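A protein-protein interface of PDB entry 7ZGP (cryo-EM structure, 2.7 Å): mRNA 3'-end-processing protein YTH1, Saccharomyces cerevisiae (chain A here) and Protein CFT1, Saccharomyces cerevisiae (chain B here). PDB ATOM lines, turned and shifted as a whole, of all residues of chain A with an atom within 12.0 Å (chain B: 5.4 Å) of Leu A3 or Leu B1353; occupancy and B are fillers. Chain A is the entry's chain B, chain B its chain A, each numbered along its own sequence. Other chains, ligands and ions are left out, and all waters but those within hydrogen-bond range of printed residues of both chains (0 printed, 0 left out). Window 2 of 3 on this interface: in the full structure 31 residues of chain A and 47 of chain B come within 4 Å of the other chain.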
ATOM      1  N   SER A   2      14.839  26.688  -9.843  1.00  0.00           N
ATOM      2  CA  SER A   2      15.274  26.176 -11.137  1.00  0.00           C
ATOM      3  C   SER A   2      14.148  25.429 -11.840  1.00  0.00           C
ATOM      4  O   SER A   2      13.554  24.511 -11.279  1.00  0.00           O
ATOM      5  CB  SER A   2      16.486  25.259 -10.969  1.00  0.00           C
ATOM      6  OG  SER A   2      16.840  24.650 -12.198  1.00  0.00           O
ATOM      7  N   LEU A   3      13.852  25.837 -13.075  1.00  0.00           N
ATOM      8  CA  LEU A   3      12.827  25.156 -13.857  1.00  0.00           C
ATOM      9  C   LEU A   3      13.320  23.825 -14.407  1.00  0.00           C
ATOM     10  O   LEU A   3      12.523  22.897 -14.580  1.00  0.00           O
ATOM     11  CB  LEU A   3      12.360  26.052 -15.005  1.00  0.00           C
ATOM     12  CG  LEU A   3      11.780  27.412 -14.619  1.00  0.00           C
ATOM     13  CD1 LEU A   3      11.691  28.310 -15.836  1.00  0.00           C
ATOM     14  CD2 LEU A   3      10.416  27.250 -13.975  1.00  0.00           C
ATOM     15  N   ILE A   4      14.619  23.717 -14.693  1.00  0.00           N
ATOM     16  CA  ILE A   4      15.161  22.482 -15.248  1.00  0.00           C
ATOM     17  C   ILE A   4      15.161  21.379 -14.199  1.00  0.00           C
ATOM     18  O   ILE A   4      14.777  20.238 -14.478  1.00  0.00           O
ATOM     19  CB  ILE A   4      16.574  22.726 -15.812  1.00  0.00           C
ATOM     20  CG1 ILE A   4      16.671  24.121 -16.432  1.00  0.00           C
ATOM     21  CG2 ILE A   4      16.929  21.661 -16.838  1.00  0.00           C
ATOM     22  CD1 ILE A   4      15.773  24.327 -17.629  1.00  0.00           C
ATOM     23  N   HIS A   5      15.586  21.700 -12.979  1.00  0.00           N
ATOM     24  CA  HIS A   5      15.642  20.746 -11.872  1.00  0.00           C
ATOM     25  C   HIS A   5      14.876  21.338 -10.699  1.00  0.00           C
ATOM     26  O   HIS A   5      15.471  21.932  -9.790  1.00  0.00           O
ATOM     27  CB  HIS A   5      17.086  20.430 -11.484  1.00  0.00           C
ATOM     28  CG  HIS A   5      17.923  19.936 -12.622  1.00  0.00           C
ATOM     29  ND1 HIS A   5      18.987  20.649 -13.127  1.00  0.00           N
ATOM     30  CD2 HIS A   5      17.850  18.800 -13.354  1.00  0.00           C
ATOM     31  CE1 HIS A   5      19.535  19.973 -14.121  1.00  0.00           C
ATOM     32  NE2 HIS A   5      18.864  18.847 -14.279  1.00  0.00           N
ATOM     33  N   PRO A   6      13.551  21.210 -10.697  1.00  0.00           N
ATOM     34  CA  PRO A   6      12.760  21.759  -9.589  1.00  0.00           C
ATOM     35  C   PRO A   6      13.134  21.114  -8.264  1.00  0.00           C
ATOM     36  O   PRO A   6      13.405  19.914  -8.187  1.00  0.00           O
ATOM     37  CB  PRO A   6      11.316  21.435  -9.988  1.00  0.00           C
ATOM     38  CG  PRO A   6      11.424  20.328 -10.979  1.00  0.00           C
ATOM     39  CD  PRO A   6      12.710  20.546 -11.706  1.00  0.00           C
ATOM     40  N   ASP A   7      13.145  21.929  -7.212  1.00  0.00           N
ATOM     41  CA  ASP A   7      13.529  21.475  -5.878  1.00  0.00           C
ATOM     42  C   ASP A   7      12.380  20.666  -5.292  1.00  0.00           C
ATOM     43  O   ASP A   7      11.448  21.219  -4.704  1.00  0.00           O
ATOM     44  CB  ASP A   7      13.882  22.662  -4.989  1.00  0.00           C
ATOM     45  CG  ASP A   7      14.647  22.253  -3.743  1.00  0.00           C
ATOM     46  OD1 ASP A   7      14.619  21.058  -3.385  1.00  0.00           O
ATOM     47  OD2 ASP A   7      15.282  23.132  -3.123  1.00  0.00           O
ATOM     48  N   THR A   8      12.445  19.347  -5.453  1.00  0.00           N
ATOM     49  CA  THR A   8      11.436  18.439  -4.925  1.00  0.00           C
ATOM     50  C   THR A   8      11.931  17.662  -3.712  1.00  0.00           C
ATOM     51  O   THR A   8      11.266  16.715  -3.281  1.00  0.00           O
ATOM     52  CB  THR A   8      10.980  17.468  -6.016  1.00  0.00           C
ATOM     53  OG1 THR A   8      12.082  16.643  -6.412  1.00  0.00           O
ATOM     54  CG2 THR A   8      10.481  18.233  -7.230  1.00  0.00           C
ATOM     55  N   VAL B 516      12.613  21.501 -21.066  1.00  0.00           N
ATOM     56  CA  VAL B 516      12.617  22.945 -20.881  1.00  0.00           C
ATOM     57  C   VAL B 516      14.057  23.427 -20.950  1.00  0.00           C
ATOM     58  O   VAL B 516      14.945  22.845 -20.314  1.00  0.00           O
ATOM     59  CB  VAL B 516      11.960  23.344 -19.549  1.00  0.00           C
ATOM     60  CG1 VAL B 516      12.252  24.798 -19.224  1.00  0.00           C
ATOM     61  CG2 VAL B 516      10.470  23.101 -19.617  1.00  0.00           C
ATOM     62  N   ASN B 535      15.590  35.947 -19.504  1.00  0.00           N
ATOM     63  CA  ASN B 535      15.296  34.894 -18.525  1.00  0.00           C
ATOM     64  C   ASN B 535      13.948  34.228 -18.798  1.00  0.00           C
ATOM     65  O   ASN B 535      13.121  34.034 -17.907  1.00  0.00           O
ATOM     66  CB  ASN B 535      15.377  35.424 -17.087  1.00  0.00           C
ATOM     67  CG  ASN B 535      14.526  36.657 -16.850  1.00  0.00           C
ATOM     68  OD1 ASN B 535      13.303  36.619 -16.975  1.00  0.00           O
ATOM     69  ND2 ASN B 535      15.173  37.759 -16.493  1.00  0.00           N
ATOM     70  N   GLU B 536      13.738  33.867 -20.061  1.00  0.00           N
ATOM     71  CA  GLU B 536      12.523  33.192 -20.498  1.00  0.00           C
ATOM     72  C   GLU B 536      12.888  31.803 -20.995  1.00  0.00           C
ATOM     73  O   GLU B 536      13.743  31.660 -21.876  1.00  0.00           O
ATOM     74  CB  GLU B 536      11.812  33.985 -21.595  1.00  0.00           C
ATOM     75  CG  GLU B 536      10.622  33.261 -22.196  1.00  0.00           C
ATOM     76  CD  GLU B 536       9.929  34.067 -23.275  1.00  0.00           C
ATOM     77  OE1 GLU B 536      10.415  34.067 -24.425  1.00  0.00           O
ATOM     78  OE2 GLU B 536       8.895  34.700 -22.974  1.00  0.00           O
ATOM     79  N   TYR B 537      12.245  30.789 -20.433  1.00  0.00           N
ATOM     80  CA  TYR B 537      12.445  29.410 -20.844  1.00  0.00           C
ATOM     81  C   TYR B 537      11.312  28.979 -21.767  1.00  0.00           C
ATOM     82  O   TYR B 537      10.238  29.582 -21.790  1.00  0.00           O
ATOM     83  CB  TYR B 537      12.526  28.487 -19.626  1.00  0.00           C
ATOM     84  CG  TYR B 537      13.792  28.660 -18.814  1.00  0.00           C
ATOM     85  CD1 TYR B 537      14.005  29.803 -18.056  1.00  0.00           C
ATOM     86  CD2 TYR B 537      14.776  27.684 -18.811  1.00  0.00           C
ATOM     87  CE1 TYR B 537      15.157  29.965 -17.316  1.00  0.00           C
ATOM     88  CE2 TYR B 537      15.933  27.839 -18.074  1.00  0.00           C
ATOM     89  CZ  TYR B 537      16.118  28.981 -17.329  1.00  0.00           C
ATOM     90  OH  TYR B 537      17.269  29.138 -16.593  1.00  0.00           O
ATOM     91  N   SER B 538      11.570  27.932 -22.545  1.00  0.00           N
ATOM     92  CA  SER B 538      10.600  27.463 -23.521  1.00  0.00           C
ATOM     93  C   SER B 538      10.613  25.945 -23.585  1.00  0.00           C
ATOM     94  O   SER B 538      11.641  25.304 -23.350  1.00  0.00           O
ATOM     95  CB  SER B 538      10.878  28.045 -24.912  1.00  0.00           C
ATOM     96  OG  SER B 538      12.201  27.761 -25.324  1.00  0.00           O
ATOM     97  N   LEU B 539       9.454  25.378 -23.904  1.00  0.00           N
ATOM     98  CA  LEU B 539       9.365  23.949 -24.171  1.00  0.00           C
ATOM     99  C   LEU B 539      10.019  23.632 -25.506  1.00  0.00           C
ATOM    100  O   LEU B 539       9.722  24.269 -26.521  1.00  0.00           O
ATOM    101  CB  LEU B 539       7.907  23.499 -24.190  1.00  0.00           C
ATOM    102  CG  LEU B 539       7.220  23.190 -22.865  1.00  0.00           C
ATOM    103  CD1 LEU B 539       5.790  22.778 -23.134  1.00  0.00           C
ATOM    104  CD2 LEU B 539       7.960  22.095 -22.130  1.00  0.00           C
ATOM    105  N   THR B 556       6.849  30.087 -25.411  1.00  0.00           N
ATOM    106  CA  THR B 556       5.825  30.662 -24.550  1.00  0.00           C
ATOM    107  C   THR B 556       5.445  32.070 -24.981  1.00  0.00           C
ATOM    108  O   THR B 556       4.367  32.550 -24.614  1.00  0.00           O
ATOM    109  CB  THR B 556       6.298  30.672 -23.095  1.00  0.00           C
ATOM    110  OG1 THR B 556       5.395  31.451 -22.301  1.00  0.00           O
ATOM    111  CG2 THR B 556       7.687  31.264 -22.998  1.00  0.00           C
ATOM    112  N   GLU B 951      21.615  22.397 -17.836  1.00  0.00           N
ATOM    113  CA  GLU B 951      21.409  23.734 -17.290  1.00  0.00           C
ATOM    114  C   GLU B 951      22.724  24.476 -17.086  1.00  0.00           C
ATOM    115  O   GLU B 951      22.813  25.676 -17.368  1.00  0.00           O
ATOM    116  CB  GLU B 951      20.633  23.648 -15.975  1.00  0.00           C
ATOM    117  CG  GLU B 951      20.193  24.993 -15.428  1.00  0.00           C
ATOM    118  CD  GLU B 951      19.355  24.868 -14.171  1.00  0.00           C
ATOM    119  OE1 GLU B 951      19.257  23.748 -13.627  1.00  0.00           O
ATOM    120  OE2 GLU B 951      18.793  25.891 -13.725  1.00  0.00           O
ATOM    121  N   LEU B1229       7.642  17.089 -15.314  1.00  0.00           N
ATOM    122  CA  LEU B1229       7.204  17.882 -14.175  1.00  0.00           C
ATOM    123  C   LEU B1229       7.684  19.314 -14.351  1.00  0.00           C
ATOM    124  O   LEU B1229       8.871  19.551 -14.596  1.00  0.00           O
ATOM    125  CB  LEU B1229       7.736  17.298 -12.866  1.00  0.00           C
ATOM    126  CG  LEU B1229       7.241  17.950 -11.575  1.00  0.00           C
ATOM    127  CD1 LEU B1229       5.987  17.263 -11.082  1.00  0.00           C
ATOM    128  CD2 LEU B1229       8.323  17.918 -10.513  1.00  0.00           C
ATOM    129  N   LEU B1230       6.762  20.264 -14.227  1.00  0.00           N
ATOM    130  CA  LEU B1230       7.086  21.663 -14.423  1.00  0.00           C
ATOM    131  C   LEU B1230       6.552  22.488 -13.261  1.00  0.00           C
ATOM    132  O   LEU B1230       5.442  22.234 -12.779  1.00  0.00           O
ATOM    133  CB  LEU B1230       6.495  22.177 -15.742  1.00  0.00           C
ATOM    134  CG  LEU B1230       7.119  23.443 -16.321  1.00  0.00           C
ATOM    135  CD1 LEU B1230       8.587  23.215 -16.612  1.00  0.00           C
ATOM    136  CD2 LEU B1230       6.386  23.868 -17.576  1.00  0.00           C
ATOM    137  N   PRO B1231       7.319  23.465 -12.781  1.00  0.00           N
ATOM    138  CA  PRO B1231       6.788  24.379 -11.766  1.00  0.00           C
ATOM    139  C   PRO B1231       5.569  25.120 -12.292  1.00  0.00           C
ATOM    140  O   PRO B1231       5.485  25.457 -13.475  1.00  0.00           O
ATOM    141  CB  PRO B1231       7.958  25.330 -11.498  1.00  0.00           C
ATOM    142  CG  PRO B1231       9.165  24.544 -11.866  1.00  0.00           C
ATOM    143  CD  PRO B1231       8.754  23.686 -13.026  1.00  0.00           C
ATOM    144  N   MET B1350       1.369  28.066 -17.110  1.00  0.00           N
ATOM    145  CA  MET B1350       2.569  27.758 -17.874  1.00  0.00           C
ATOM    146  C   MET B1350       3.557  28.915 -17.916  1.00  0.00           C
ATOM    147  O   MET B1350       4.624  28.775 -18.522  1.00  0.00           O
ATOM    148  CB  MET B1350       2.183  27.359 -19.300  1.00  0.00           C
ATOM    149  CG  MET B1350       1.861  25.886 -19.458  1.00  0.00           C
ATOM    150  SD  MET B1350       3.268  24.831 -19.095  1.00  0.00           S
ATOM    151  CE  MET B1350       3.616  24.199 -20.729  1.00  0.00           C
ATOM    152  N   ARG B1351       3.232  30.044 -17.293  1.00  0.00           N
ATOM    153  CA  ARG B1351       4.078  31.229 -17.341  1.00  0.00           C
ATOM    154  C   ARG B1351       5.185  31.214 -16.298  1.00  0.00           C
ATOM    155  O   ARG B1351       5.852  32.237 -16.113  1.00  0.00           O
ATOM    156  CB  ARG B1351       3.223  32.486 -17.184  1.00  0.00           C
ATOM    157  CG  ARG B1351       2.204  32.648 -18.291  1.00  0.00           C
ATOM    158  CD  ARG B1351       1.860  34.101 -18.531  1.00  0.00           C
ATOM    159  NE  ARG B1351       0.959  34.248 -19.667  1.00  0.00           N
ATOM    160  CZ  ARG B1351       0.284  35.354 -19.950  1.00  0.00           C
ATOM    161  NH1 ARG B1351       0.383  36.435 -19.195  1.00  0.00           N
ATOM    162  NH2 ARG B1351      -0.511  35.373 -21.015  1.00  0.00           N
ATOM    163  N   SER B1352       5.391  30.090 -15.609  1.00  0.00           N
ATOM    164  CA  SER B1352       6.592  29.936 -14.802  1.00  0.00           C
ATOM    165  C   SER B1352       7.847  29.913 -15.663  1.00  0.00           C
ATOM    166  O   SER B1352       8.939  30.188 -15.158  1.00  0.00           O
ATOM    167  CB  SER B1352       6.505  28.661 -13.964  1.00  0.00           C
ATOM    168  OG  SER B1352       6.128  27.553 -14.761  1.00  0.00           O
ATOM    169  N   LEU B1353       7.708  29.594 -16.952  1.00  0.00           N
ATOM    170  CA  LEU B1353       8.829  29.673 -17.877  1.00  0.00           C
ATOM    171  C   LEU B1353       9.231  31.111 -18.169  1.00  0.00           C
ATOM    172  O   LEU B1353      10.364  31.351 -18.598  1.00  0.00           O
ATOM    173  CB  LEU B1353       8.479  28.957 -19.182  1.00  0.00           C
ATOM    174  CG  LEU B1353       7.916  27.541 -19.053  1.00  0.00           C
ATOM    175  CD1 LEU B1353       7.227  27.117 -20.337  1.00  0.00           C
ATOM    176  CD2 LEU B1353       9.020  26.565 -18.694  1.00  0.00           C
ATOM    177  N   CYS B1354       8.331  32.071 -17.944  1.00  0.00           N
ATOM    178  CA  CYS B1354       8.640  33.469 -18.209  1.00  0.00           C
ATOM    179  C   CYS B1354       9.535  34.080 -17.139  1.00  0.00           C
ATOM    180  O   CYS B1354      10.097  35.157 -17.361  1.00  0.00           O
ATOM    181  CB  CYS B1354       7.348  34.278 -18.328  1.00  0.00           C
ATOM    182  SG  CYS B1354       6.241  33.726 -19.642  1.00  0.00           S
ATOM    183  N   GLN B1355       9.677  33.427 -15.988  1.00  0.00           N
ATOM    184  CA  GLN B1355      10.551  33.897 -14.921  1.00  0.00           C
ATOM    185  C   GLN B1355      11.415  32.738 -14.446  1.00  0.00           C
ATOM    186  O   GLN B1355      10.910  31.796 -13.828  1.00  0.00           O
ATOM    187  CB  GLN B1355       9.743  34.493 -13.762  1.00  0.00           C
ATOM    188  CG  GLN B1355       8.546  33.663 -13.320  1.00  0.00           C
ATOM    189  CD  GLN B1355       7.227  34.236 -13.798  1.00  0.00           C
ATOM    190  OE1 GLN B1355       7.194  35.161 -14.609  1.00  0.00           O
ATOM    191  NE2 GLN B1355       6.127  33.688 -13.294  1.00  0.00           N
ATOM    192  N   GLY B1356      12.710  32.805 -14.739  1.00  0.00           N
ATOM    193  CA  GLY B1356      13.623  31.757 -14.331  1.00  0.00           C
ATOM    194  C   GLY B1356      15.076  32.183 -14.342  1.00  0.00           C
ATOM    195  O   GLY B1356      15.548  32.769 -15.321  1.00  0.00           O
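A ring nitrogen (ND1) of His A5 lies within hydrogen-bond range of the side-chain carboxylate of Glu B951, at 3.2 Å.
The side-chain carboxylate (OE2) of Glu B951 is in hydrogen-bond range of the side-chain hydroxyl (OG) of Ser A2 (2.8 Å).
O of Pro B1231 lies within hydrogen-bond range of OG of Ser B1352 (2.5 Å).
The side-chain hydroxyl (OG) of Ser A2 lies within hydrogen-bond range of the backbone NH (N) of His A5.
N of Ile A4 lies close to OG of Ser A2, 3.5 Å away.
O of Leu B1353 sits at hydrogen-bond distance from N of Tyr B537, at 2.7 Å.
Tyr B537 touches Leu A3.
Pro B1231 touches Leu A3 (CG to CD2, 3.7 Å).
Ser B1352 touches Leu A3.
Leu A3 touches Leu B1353.
CD1 of Ile A4 touches O of Val B516, at 3.2 Å.
Tyr B537 touches Ile A4 (CE2 to CD1, 3.5 Å).
Ile A4 touches Glu B951 (CG1 to CD, 3.6 Å).
Leu B1229 touches Pro A6 (CD2 to CG, 3.95 Å).
Thr A8 touches Leu B1229.
Leu A3 touches just these residues of chain B: Tyr B537, Pro B1231, Ser B1352 and Leu B1353.
Of chain A, only Leu A3 (3.8 Å) comes within 4 Å of Leu B1353.
Val B516 touches just one residue of chain A: Ile A4.
Glu B536 touches none of the printed residues of chain A.
Tyr B537 touches just these residues of chain A: Leu A3 (3.5 Å) and Ile A4 (3.5 Å).
No residue of chain A comes within 4 Å of Ser B538.
No residue of chain A comes within 4 Å of Leu B539.
No residue of chain A comes within 4 Å of Thr B556.
No residue of chain A comes within 4 Å of Leu B1230.
Pro B1231 touches one residue of chain A.
No residue of chain A comes within 4 Å of Met B1350.
Ser B1352 touches just one residue of chain A: Leu A3 (3.4 Å).
No residue of chain A comes within 4 Å of Cys B1354.
No residue of chain A comes within 4 Å of Gln B1355.
Of the printed residues of chain A, Glu B951 touches Ser A2, Ile A4 and His A5.
Printed residues of chain B within 4 Å of Thr A8: Leu B1229 (3.9 Å).
Arg B1351 touches none of the printed residues of chain A.
Asn B535 touches none of the printed residues of chain A.
The nearest residue of chain B that does not touch Leu A3 is Gln B1355 (4.1 Å).
The nearest residue of chain A that does not touch Leu B1353 is Ile A4 (7.2 Å).
The nearest printed residue of chain A that does not touch Leu B1229 is Leu A3 (5.0 Å).
Of the 7 printed residues of chain A, 6 touch a printed residue of chain B.
Hydrophobic or aromatic side chains of chain B within 4 Å of the printed part of chain A: Val B516, Tyr B537, Leu B1229 and Pro B1231.
Among the printed residues, 11 pairs touch across the chains.
Among the printed residues, no Asp or Glu carboxylate lies within 4 Å of a Lys or Arg side-chain nitrogen of the other chain.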
